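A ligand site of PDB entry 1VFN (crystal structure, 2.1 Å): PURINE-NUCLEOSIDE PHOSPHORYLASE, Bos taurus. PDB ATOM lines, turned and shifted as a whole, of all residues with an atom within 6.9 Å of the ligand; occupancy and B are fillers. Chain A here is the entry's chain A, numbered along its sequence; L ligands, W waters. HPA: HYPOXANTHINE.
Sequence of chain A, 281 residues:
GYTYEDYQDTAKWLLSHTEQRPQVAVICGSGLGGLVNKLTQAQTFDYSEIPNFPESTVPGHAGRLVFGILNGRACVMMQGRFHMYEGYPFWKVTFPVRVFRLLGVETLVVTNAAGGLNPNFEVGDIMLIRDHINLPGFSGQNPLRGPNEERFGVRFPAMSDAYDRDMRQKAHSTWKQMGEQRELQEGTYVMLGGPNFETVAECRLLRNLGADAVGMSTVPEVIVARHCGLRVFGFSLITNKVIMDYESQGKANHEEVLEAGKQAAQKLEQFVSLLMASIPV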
ATOM      1  N   SER A  30     -21.692 -24.849 -21.456  1.00  0.00           N
ATOM      2  CA  SER A  30     -21.847 -23.425 -21.902  1.00  0.00           C
ATOM      3  C   SER A  30     -22.913 -23.200 -22.994  1.00  0.00           C
ATOM      4  O   SER A  30     -22.588 -23.183 -24.210  1.00  0.00           O
ATOM      5  CB  SER A  30     -20.489 -22.690 -22.206  1.00  0.00           C
ATOM      6  OG  SER A  30     -20.177 -21.628 -21.291  1.00  0.00           O
ATOM      7  N   ALA A 113     -18.583 -25.535 -25.852  1.00  0.00           N
ATOM      8  CA  ALA A 113     -18.540 -24.438 -26.819  1.00  0.00           C
ATOM      9  C   ALA A 113     -17.069 -24.010 -26.857  1.00  0.00           C
ATOM     10  O   ALA A 113     -16.401 -24.073 -25.845  1.00  0.00           O
ATOM     11  CB  ALA A 113     -19.377 -23.269 -26.353  1.00  0.00           C
ATOM     12  N   ALA A 114     -16.554 -23.628 -28.022  1.00  0.00           N
ATOM     13  CA  ALA A 114     -15.171 -23.256 -28.086  1.00  0.00           C
ATOM     14  C   ALA A 114     -14.944 -22.305 -29.187  1.00  0.00           C
ATOM     15  O   ALA A 114     -15.774 -22.139 -30.125  1.00  0.00           O
ATOM     16  CB  ALA A 114     -14.332 -24.493 -28.419  1.00  0.00           C
ATOM     17  N   GLY A 115     -13.811 -21.649 -29.063  1.00  0.00           N
ATOM     18  CA  GLY A 115     -13.443 -20.704 -30.135  1.00  0.00           C
ATOM     19  C   GLY A 115     -12.660 -21.446 -31.210  1.00  0.00           C
ATOM     20  O   GLY A 115     -11.827 -22.289 -30.900  1.00  0.00           O
ATOM     21  N   GLY A 116     -12.938 -21.165 -32.498  1.00  0.00           N
ATOM     22  CA  GLY A 116     -12.259 -21.842 -33.573  1.00  0.00           C
ATOM     23  C   GLY A 116     -10.904 -21.205 -33.896  1.00  0.00           C
ATOM     24  O   GLY A 116     -10.788 -19.989 -34.066  1.00  0.00           O
ATOM     25  N   TYR A 189      -8.580 -30.141 -29.492  1.00  0.00           N
ATOM     26  CA  TYR A 189      -9.114 -29.152 -28.566  1.00  0.00           C
ATOM     27  C   TYR A 189      -8.023 -28.823 -27.596  1.00  0.00           C
ATOM     28  O   TYR A 189      -7.322 -29.718 -27.084  1.00  0.00           O
ATOM     29  CB  TYR A 189     -10.367 -29.731 -27.858  1.00  0.00           C
ATOM     30  CG  TYR A 189     -10.980 -28.833 -26.763  1.00  0.00           C
ATOM     31  CD1 TYR A 189     -10.543 -28.964 -25.433  1.00  0.00           C
ATOM     32  CD2 TYR A 189     -12.000 -27.897 -27.031  1.00  0.00           C
ATOM     33  CE1 TYR A 189     -11.083 -28.184 -24.419  1.00  0.00           C
ATOM     34  CE2 TYR A 189     -12.570 -27.121 -26.020  1.00  0.00           C
ATOM     35  CZ  TYR A 189     -12.083 -27.270 -24.718  1.00  0.00           C
ATOM     36  OH  TYR A 189     -12.637 -26.580 -23.703  1.00  0.00           O
ATOM     37  N   LEU A 192      -7.183 -24.152 -21.732  1.00  0.00           N
ATOM     38  CA  LEU A 192      -6.433 -23.157 -20.978  1.00  0.00           C
ATOM     39  C   LEU A 192      -7.286 -22.774 -19.793  1.00  0.00           C
ATOM     40  O   LEU A 192      -8.449 -23.127 -19.762  1.00  0.00           O
ATOM     41  CB  LEU A 192      -5.872 -21.973 -21.746  1.00  0.00           C
ATOM     42  CG  LEU A 192      -6.671 -21.604 -22.933  1.00  0.00           C
ATOM     43  CD1 LEU A 192      -8.051 -21.080 -22.430  1.00  0.00           C
ATOM     44  CD2 LEU A 192      -5.918 -20.474 -23.603  1.00  0.00           C
ATOM     45  N   ASN A 196     -10.495 -14.988 -18.845  1.00  0.00           N
ATOM     46  CA  ASN A 196     -10.498 -13.992 -19.875  1.00  0.00           C
ATOM     47  C   ASN A 196     -10.267 -14.676 -21.158  1.00  0.00           C
ATOM     48  O   ASN A 196      -9.767 -15.810 -21.175  1.00  0.00           O
ATOM     49  CB  ASN A 196      -9.335 -13.007 -19.680  1.00  0.00           C
ATOM     50  CG  ASN A 196      -8.009 -13.647 -19.947  1.00  0.00           C
ATOM     51  OD1 ASN A 196      -7.483 -13.579 -21.074  1.00  0.00           O
ATOM     52  ND2 ASN A 196      -7.488 -14.308 -18.938  1.00  0.00           N
ATOM     53  N   PHE A 197     -10.626 -13.985 -22.191  1.00  0.00           N
ATOM     54  CA  PHE A 197     -10.449 -14.435 -23.538  1.00  0.00           C
ATOM     55  C   PHE A 197      -9.003 -14.123 -23.938  1.00  0.00           C
ATOM     56  O   PHE A 197      -8.355 -13.293 -23.311  1.00  0.00           O
ATOM     57  CB  PHE A 197     -11.528 -13.789 -24.426  1.00  0.00           C
ATOM     58  CG  PHE A 197     -12.878 -14.444 -24.198  1.00  0.00           C
ATOM     59  CD1 PHE A 197     -13.024 -15.823 -24.212  1.00  0.00           C
ATOM     60  CD2 PHE A 197     -14.031 -13.674 -24.018  1.00  0.00           C
ATOM     61  CE1 PHE A 197     -14.282 -16.413 -24.077  1.00  0.00           C
ATOM     62  CE2 PHE A 197     -15.302 -14.235 -23.857  1.00  0.00           C
ATOM     63  CZ  PHE A 197     -15.426 -15.623 -23.877  1.00  0.00           C
ATOM     64  N   GLU A 198      -8.520 -14.806 -24.974  1.00  0.00           N
ATOM     65  CA  GLU A 198      -7.166 -14.732 -25.438  1.00  0.00           C
ATOM     66  C   GLU A 198      -6.844 -13.550 -26.222  1.00  0.00           C
ATOM     67  O   GLU A 198      -7.705 -12.986 -26.855  1.00  0.00           O
ATOM     68  CB  GLU A 198      -6.897 -15.919 -26.377  1.00  0.00           C
ATOM     69  CG  GLU A 198      -7.205 -17.310 -25.765  1.00  0.00           C
ATOM     70  CD  GLU A 198      -8.691 -17.614 -25.550  1.00  0.00           C
ATOM     71  OE1 GLU A 198      -9.567 -17.405 -26.346  1.00  0.00           O
ATOM     72  OE2 GLU A 198      -8.928 -18.202 -24.432  1.00  0.00           O
ATOM     73  N   CYS A 203      -3.548 -16.473 -29.403  1.00  0.00           N
ATOM     74  CA  CYS A 203      -4.232 -17.282 -30.383  1.00  0.00           C
ATOM     75  C   CYS A 203      -3.301 -17.796 -31.425  1.00  0.00           C
ATOM     76  O   CYS A 203      -3.373 -18.936 -31.808  1.00  0.00           O
ATOM     77  CB  CYS A 203      -5.405 -16.543 -31.021  1.00  0.00           C
ATOM     78  SG  CYS A 203      -6.833 -16.290 -29.879  1.00  0.00           S
ATOM     79  N   VAL A 214     -10.372 -23.771 -28.968  1.00  0.00           N
ATOM     80  CA  VAL A 214      -9.895 -23.487 -27.631  1.00  0.00           C
ATOM     81  C   VAL A 214     -11.070 -23.270 -26.679  1.00  0.00           C
ATOM     82  O   VAL A 214     -12.068 -22.654 -27.021  1.00  0.00           O
ATOM     83  CB  VAL A 214      -9.006 -22.237 -27.719  1.00  0.00           C
ATOM     84  CG1 VAL A 214      -9.803 -21.082 -28.360  1.00  0.00           C
ATOM     85  CG2 VAL A 214      -8.563 -21.753 -26.348  1.00  0.00           C
ATOM     86  N   GLY A 215     -10.939 -23.792 -25.489  1.00  0.00           N
ATOM     87  CA  GLY A 215     -11.953 -23.632 -24.491  1.00  0.00           C
ATOM     88  C   GLY A 215     -11.329 -23.724 -23.089  1.00  0.00           C
ATOM     89  O   GLY A 215     -10.105 -23.850 -22.919  1.00  0.00           O
ATOM     90  N   MET A 216     -12.182 -23.663 -22.086  1.00  0.00           N
ATOM     91  CA  MET A 216     -11.828 -23.662 -20.666  1.00  0.00           C
ATOM     92  C   MET A 216     -12.374 -24.834 -19.857  1.00  0.00           C
ATOM     93  O   MET A 216     -12.415 -24.711 -18.624  1.00  0.00           O
ATOM     94  CB  MET A 216     -12.319 -22.342 -20.050  1.00  0.00           C
ATOM     95  CG  MET A 216     -11.848 -21.156 -20.874  1.00  0.00           C
ATOM     96  SD  MET A 216     -12.431 -19.541 -20.350  1.00  0.00           S
ATOM     97  CE  MET A 216     -14.029 -20.098 -19.916  1.00  0.00           C
ATOM     98  N   LEU A 237     -18.887 -27.219 -29.991  1.00  0.00           N
ATOM     99  CA  LEU A 237     -19.689 -26.390 -30.852  1.00  0.00           C
ATOM    100  C   LEU A 237     -18.802 -25.172 -31.044  1.00  0.00           C
ATOM    101  O   LEU A 237     -18.456 -24.541 -30.055  1.00  0.00           O
ATOM    102  CB  LEU A 237     -20.966 -25.887 -30.163  1.00  0.00           C
ATOM    103  CG  LEU A 237     -22.142 -25.382 -31.039  1.00  0.00           C
ATOM    104  CD1 LEU A 237     -22.769 -24.112 -30.487  1.00  0.00           C
ATOM    105  CD2 LEU A 237     -21.852 -25.305 -32.541  1.00  0.00           C
ATOM    106  N   ILE A 238     -18.440 -24.847 -32.259  1.00  0.00           N
ATOM    107  CA  ILE A 238     -17.592 -23.686 -32.553  1.00  0.00           C
ATOM    108  C   ILE A 238     -18.376 -22.324 -32.533  1.00  0.00           C
ATOM    109  O   ILE A 238     -19.427 -22.200 -33.122  1.00  0.00           O
ATOM    110  CB  ILE A 238     -16.846 -23.850 -33.876  1.00  0.00           C
ATOM    111  CG1 ILE A 238     -15.903 -25.052 -33.764  1.00  0.00           C
ATOM    112  CG2 ILE A 238     -16.065 -22.597 -34.236  1.00  0.00           C
ATOM    113  CD1 ILE A 238     -15.079 -25.029 -32.483  1.00  0.00           C
ATOM    114  N   THR A 239     -17.849 -21.301 -31.869  1.00  0.00           N
ATOM    115  CA  THR A 239     -18.508 -19.999 -31.813  1.00  0.00           C
ATOM    116  C   THR A 239     -17.664 -18.717 -32.131  1.00  0.00           C
ATOM    117  O   THR A 239     -18.254 -17.711 -31.900  1.00  0.00           O
ATOM    118  CB  THR A 239     -19.232 -19.967 -30.430  1.00  0.00           C
ATOM    119  OG1 THR A 239     -18.369 -20.163 -29.277  1.00  0.00           O
ATOM    120  CG2 THR A 239     -20.101 -21.183 -30.329  1.00  0.00           C
ATOM    121  N   ASN A 240     -16.340 -18.711 -32.629  1.00  0.00           N
ATOM    122  CA  ASN A 240     -15.584 -17.432 -32.864  1.00  0.00           C
ATOM    123  C   ASN A 240     -14.441 -17.194 -33.991  1.00  0.00           C
ATOM    124  O   ASN A 240     -14.753 -17.556 -35.070  1.00  0.00           O
ATOM    125  CB  ASN A 240     -15.814 -16.433 -31.693  1.00  0.00           C
ATOM    126  CG  ASN A 240     -15.455 -16.999 -30.316  1.00  0.00           C
ATOM    127  OD1 ASN A 240     -16.125 -17.884 -29.753  1.00  0.00           O
ATOM    128  ND2 ASN A 240     -14.356 -16.487 -29.782  1.00  0.00           N
ATOM    129  N   LYS A 241     -13.148 -16.569 -33.971  1.00  0.00           N
ATOM    130  CA  LYS A 241     -12.176 -15.996 -32.999  1.00  0.00           C
ATOM    131  C   LYS A 241     -10.954 -15.155 -33.594  1.00  0.00           C
ATOM    132  O   LYS A 241     -10.351 -15.515 -34.605  1.00  0.00           O
ATOM    133  CB  LYS A 241     -11.533 -17.208 -32.433  1.00  0.00           C
ATOM    134  CG  LYS A 241     -11.355 -17.231 -30.926  1.00  0.00           C
ATOM    135  CD  LYS A 241      -9.946 -17.642 -30.776  1.00  0.00           C
ATOM    136  CE  LYS A 241      -9.236 -16.901 -31.870  1.00  0.00           C
ATOM    137  NZ  LYS A 241      -8.818 -17.769 -32.962  1.00  0.00           N
ATOM    138  N   VAL A 242     -10.513 -14.070 -32.882  1.00  0.00           N
ATOM    139  CA  VAL A 242      -9.499 -13.027 -33.242  1.00  0.00           C
ATOM    140  C   VAL A 242      -8.009 -13.219 -33.506  1.00  0.00           C
ATOM    141  O   VAL A 242      -7.239 -13.380 -32.597  1.00  0.00           O
ATOM    142  CB  VAL A 242      -9.778 -11.638 -32.660  1.00  0.00           C
ATOM    143  CG1 VAL A 242      -8.944 -10.597 -33.427  1.00  0.00           C
ATOM    144  CG2 VAL A 242     -11.256 -11.251 -32.782  1.00  0.00           C
ATOM    145  N   ALA A 252     -13.972 -10.935 -28.502  1.00  0.00           N
ATOM    146  CA  ALA A 252     -14.808 -12.084 -28.127  1.00  0.00           C
ATOM    147  C   ALA A 252     -15.816 -11.694 -27.036  1.00  0.00           C
ATOM    148  O   ALA A 252     -15.500 -10.930 -26.139  1.00  0.00           O
ATOM    149  CB  ALA A 252     -14.038 -13.356 -27.808  1.00  0.00           C
ATOM    150  N   ASN A 253     -17.052 -12.207 -27.128  1.00  0.00           N
ATOM    151  CA  ASN A 253     -18.140 -11.905 -26.199  1.00  0.00           C
ATOM    152  C   ASN A 253     -18.811 -13.124 -25.578  1.00  0.00           C
ATOM    153  O   ASN A 253     -19.107 -14.103 -26.241  1.00  0.00           O
ATOM    154  CB  ASN A 253     -19.310 -11.280 -27.042  1.00  0.00           C
ATOM    155  CG  ASN A 253     -19.077  -9.882 -27.441  1.00  0.00           C
ATOM    156  OD1 ASN A 253     -18.997  -9.006 -26.565  1.00  0.00           O
ATOM    157  ND2 ASN A 253     -18.990  -9.674 -28.744  1.00  0.00           N
ATOM    158  N   GLU A 256     -22.435 -15.111 -27.115  1.00  0.00           N
ATOM    159  CA  GLU A 256     -22.099 -16.045 -28.147  1.00  0.00           C
ATOM    160  C   GLU A 256     -22.398 -17.348 -27.406  1.00  0.00           C
ATOM    161  O   GLU A 256     -21.739 -18.367 -27.435  1.00  0.00           O
ATOM    162  CB  GLU A 256     -20.677 -15.869 -28.681  1.00  0.00           C
ATOM    163  CG  GLU A 256     -20.355 -14.511 -29.398  1.00  0.00           C
ATOM    164  CD  GLU A 256     -18.872 -14.274 -29.770  1.00  0.00           C
ATOM    165  OE1 GLU A 256     -17.898 -14.636 -29.079  1.00  0.00           O
ATOM    166  OE2 GLU A 256     -18.718 -13.628 -30.918  1.00  0.00           O
HETATM  167  N1  HPA L   1     -11.883 -18.653 -26.253  1.00  0.00           N
HETATM  168  C2  HPA L   1     -11.930 -19.470 -25.128  1.00  0.00           C
HETATM  169  N3  HPA L   1     -13.004 -20.189 -24.742  1.00  0.00           N
HETATM  170  C4  HPA L   1     -14.018 -20.052 -25.614  1.00  0.00           C
HETATM  171  C5  HPA L   1     -14.087 -19.232 -26.736  1.00  0.00           C
HETATM  172  C6  HPA L   1     -12.970 -18.425 -27.110  1.00  0.00           C
HETATM  173  O6  HPA L   1     -12.845 -17.676 -28.085  1.00  0.00           O
HETATM  174  N7  HPA L   1     -15.348 -19.331 -27.345  1.00  0.00           N
HETATM  175  C8  HPA L   1     -15.982 -20.189 -26.591  1.00  0.00           C
HETATM  176  N9  HPA L   1     -15.245 -20.672 -25.506  1.00  0.00           N
HETATM  177  O   HOH W   1     -10.896 -15.491 -27.902  1.00  0.00           O
HETATM  178  O   HOH W   2     -14.557 -21.874 -22.979  1.00  0.00           O
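The side-chain amide nitrogen of Asn 240 is in hydrogen-bond range of an oxygen (O6) of the ligand (2.6 Å). The side-chain carboxylate of Glu 198 lies within hydrogen-bond range of a nitrogen (N1) of the ligand (2.6 Å). The backbone NH (N) of Gly 115 sits close to a nitrogen (N7) of the ligand, at 3.3 Å. The backbone carbonyl oxygen (O) of Val 214 sits close to a nitrogen (N3) of the ligand (3.5 Å).
OD1 of Asn 240 sits close to OG1 of Thr 239 (3.2 Å). The side-chain amino group of Lys 241 sits at hydrogen-bond distance from the backbone carbonyl oxygen of Gly 116. The backbone carbonyl oxygen (O) of Gly 115 sits at hydrogen-bond distance from the backbone NH (N) of Val 214 (2.8 Å). The backbone carbonyl oxygen (O) of Ala 114 lies within hydrogen-bond range of the backbone NH (N) of Thr 239. The backbone NH (N) of Ala 114 is in hydrogen-bond range of the backbone carbonyl oxygen (O) of Leu 237 (2.9 Å). The backbone NH of Leu 192 is in hydrogen-bond range of the backbone carbonyl oxygen of Gly 215.
Merely in contact with the ligand: Ala 113 (3.6 Å), Ala 114 (3.5 Å), Phe 197 (3.7 Å), Gly 215 (3.6 Å), Thr 239 (3.6 Å) and Lys 241 (3.2 Å). Of the 23 residues printed, 10 come within 4 Å of the ligand. The nearest printed residue that does not touch the ligand is Met 216 (4.2 Å).
Water W2 lies within hydrogen-bond range of N9 of the ligand (2.9 Å) and N of Met 216 (3.1 Å). Water W1 lies within hydrogen-bond range of the side-chain carboxylate (OE1) of Glu 198 (2.8 Å) and an oxygen (O6) of the ligand (2.9 Å).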
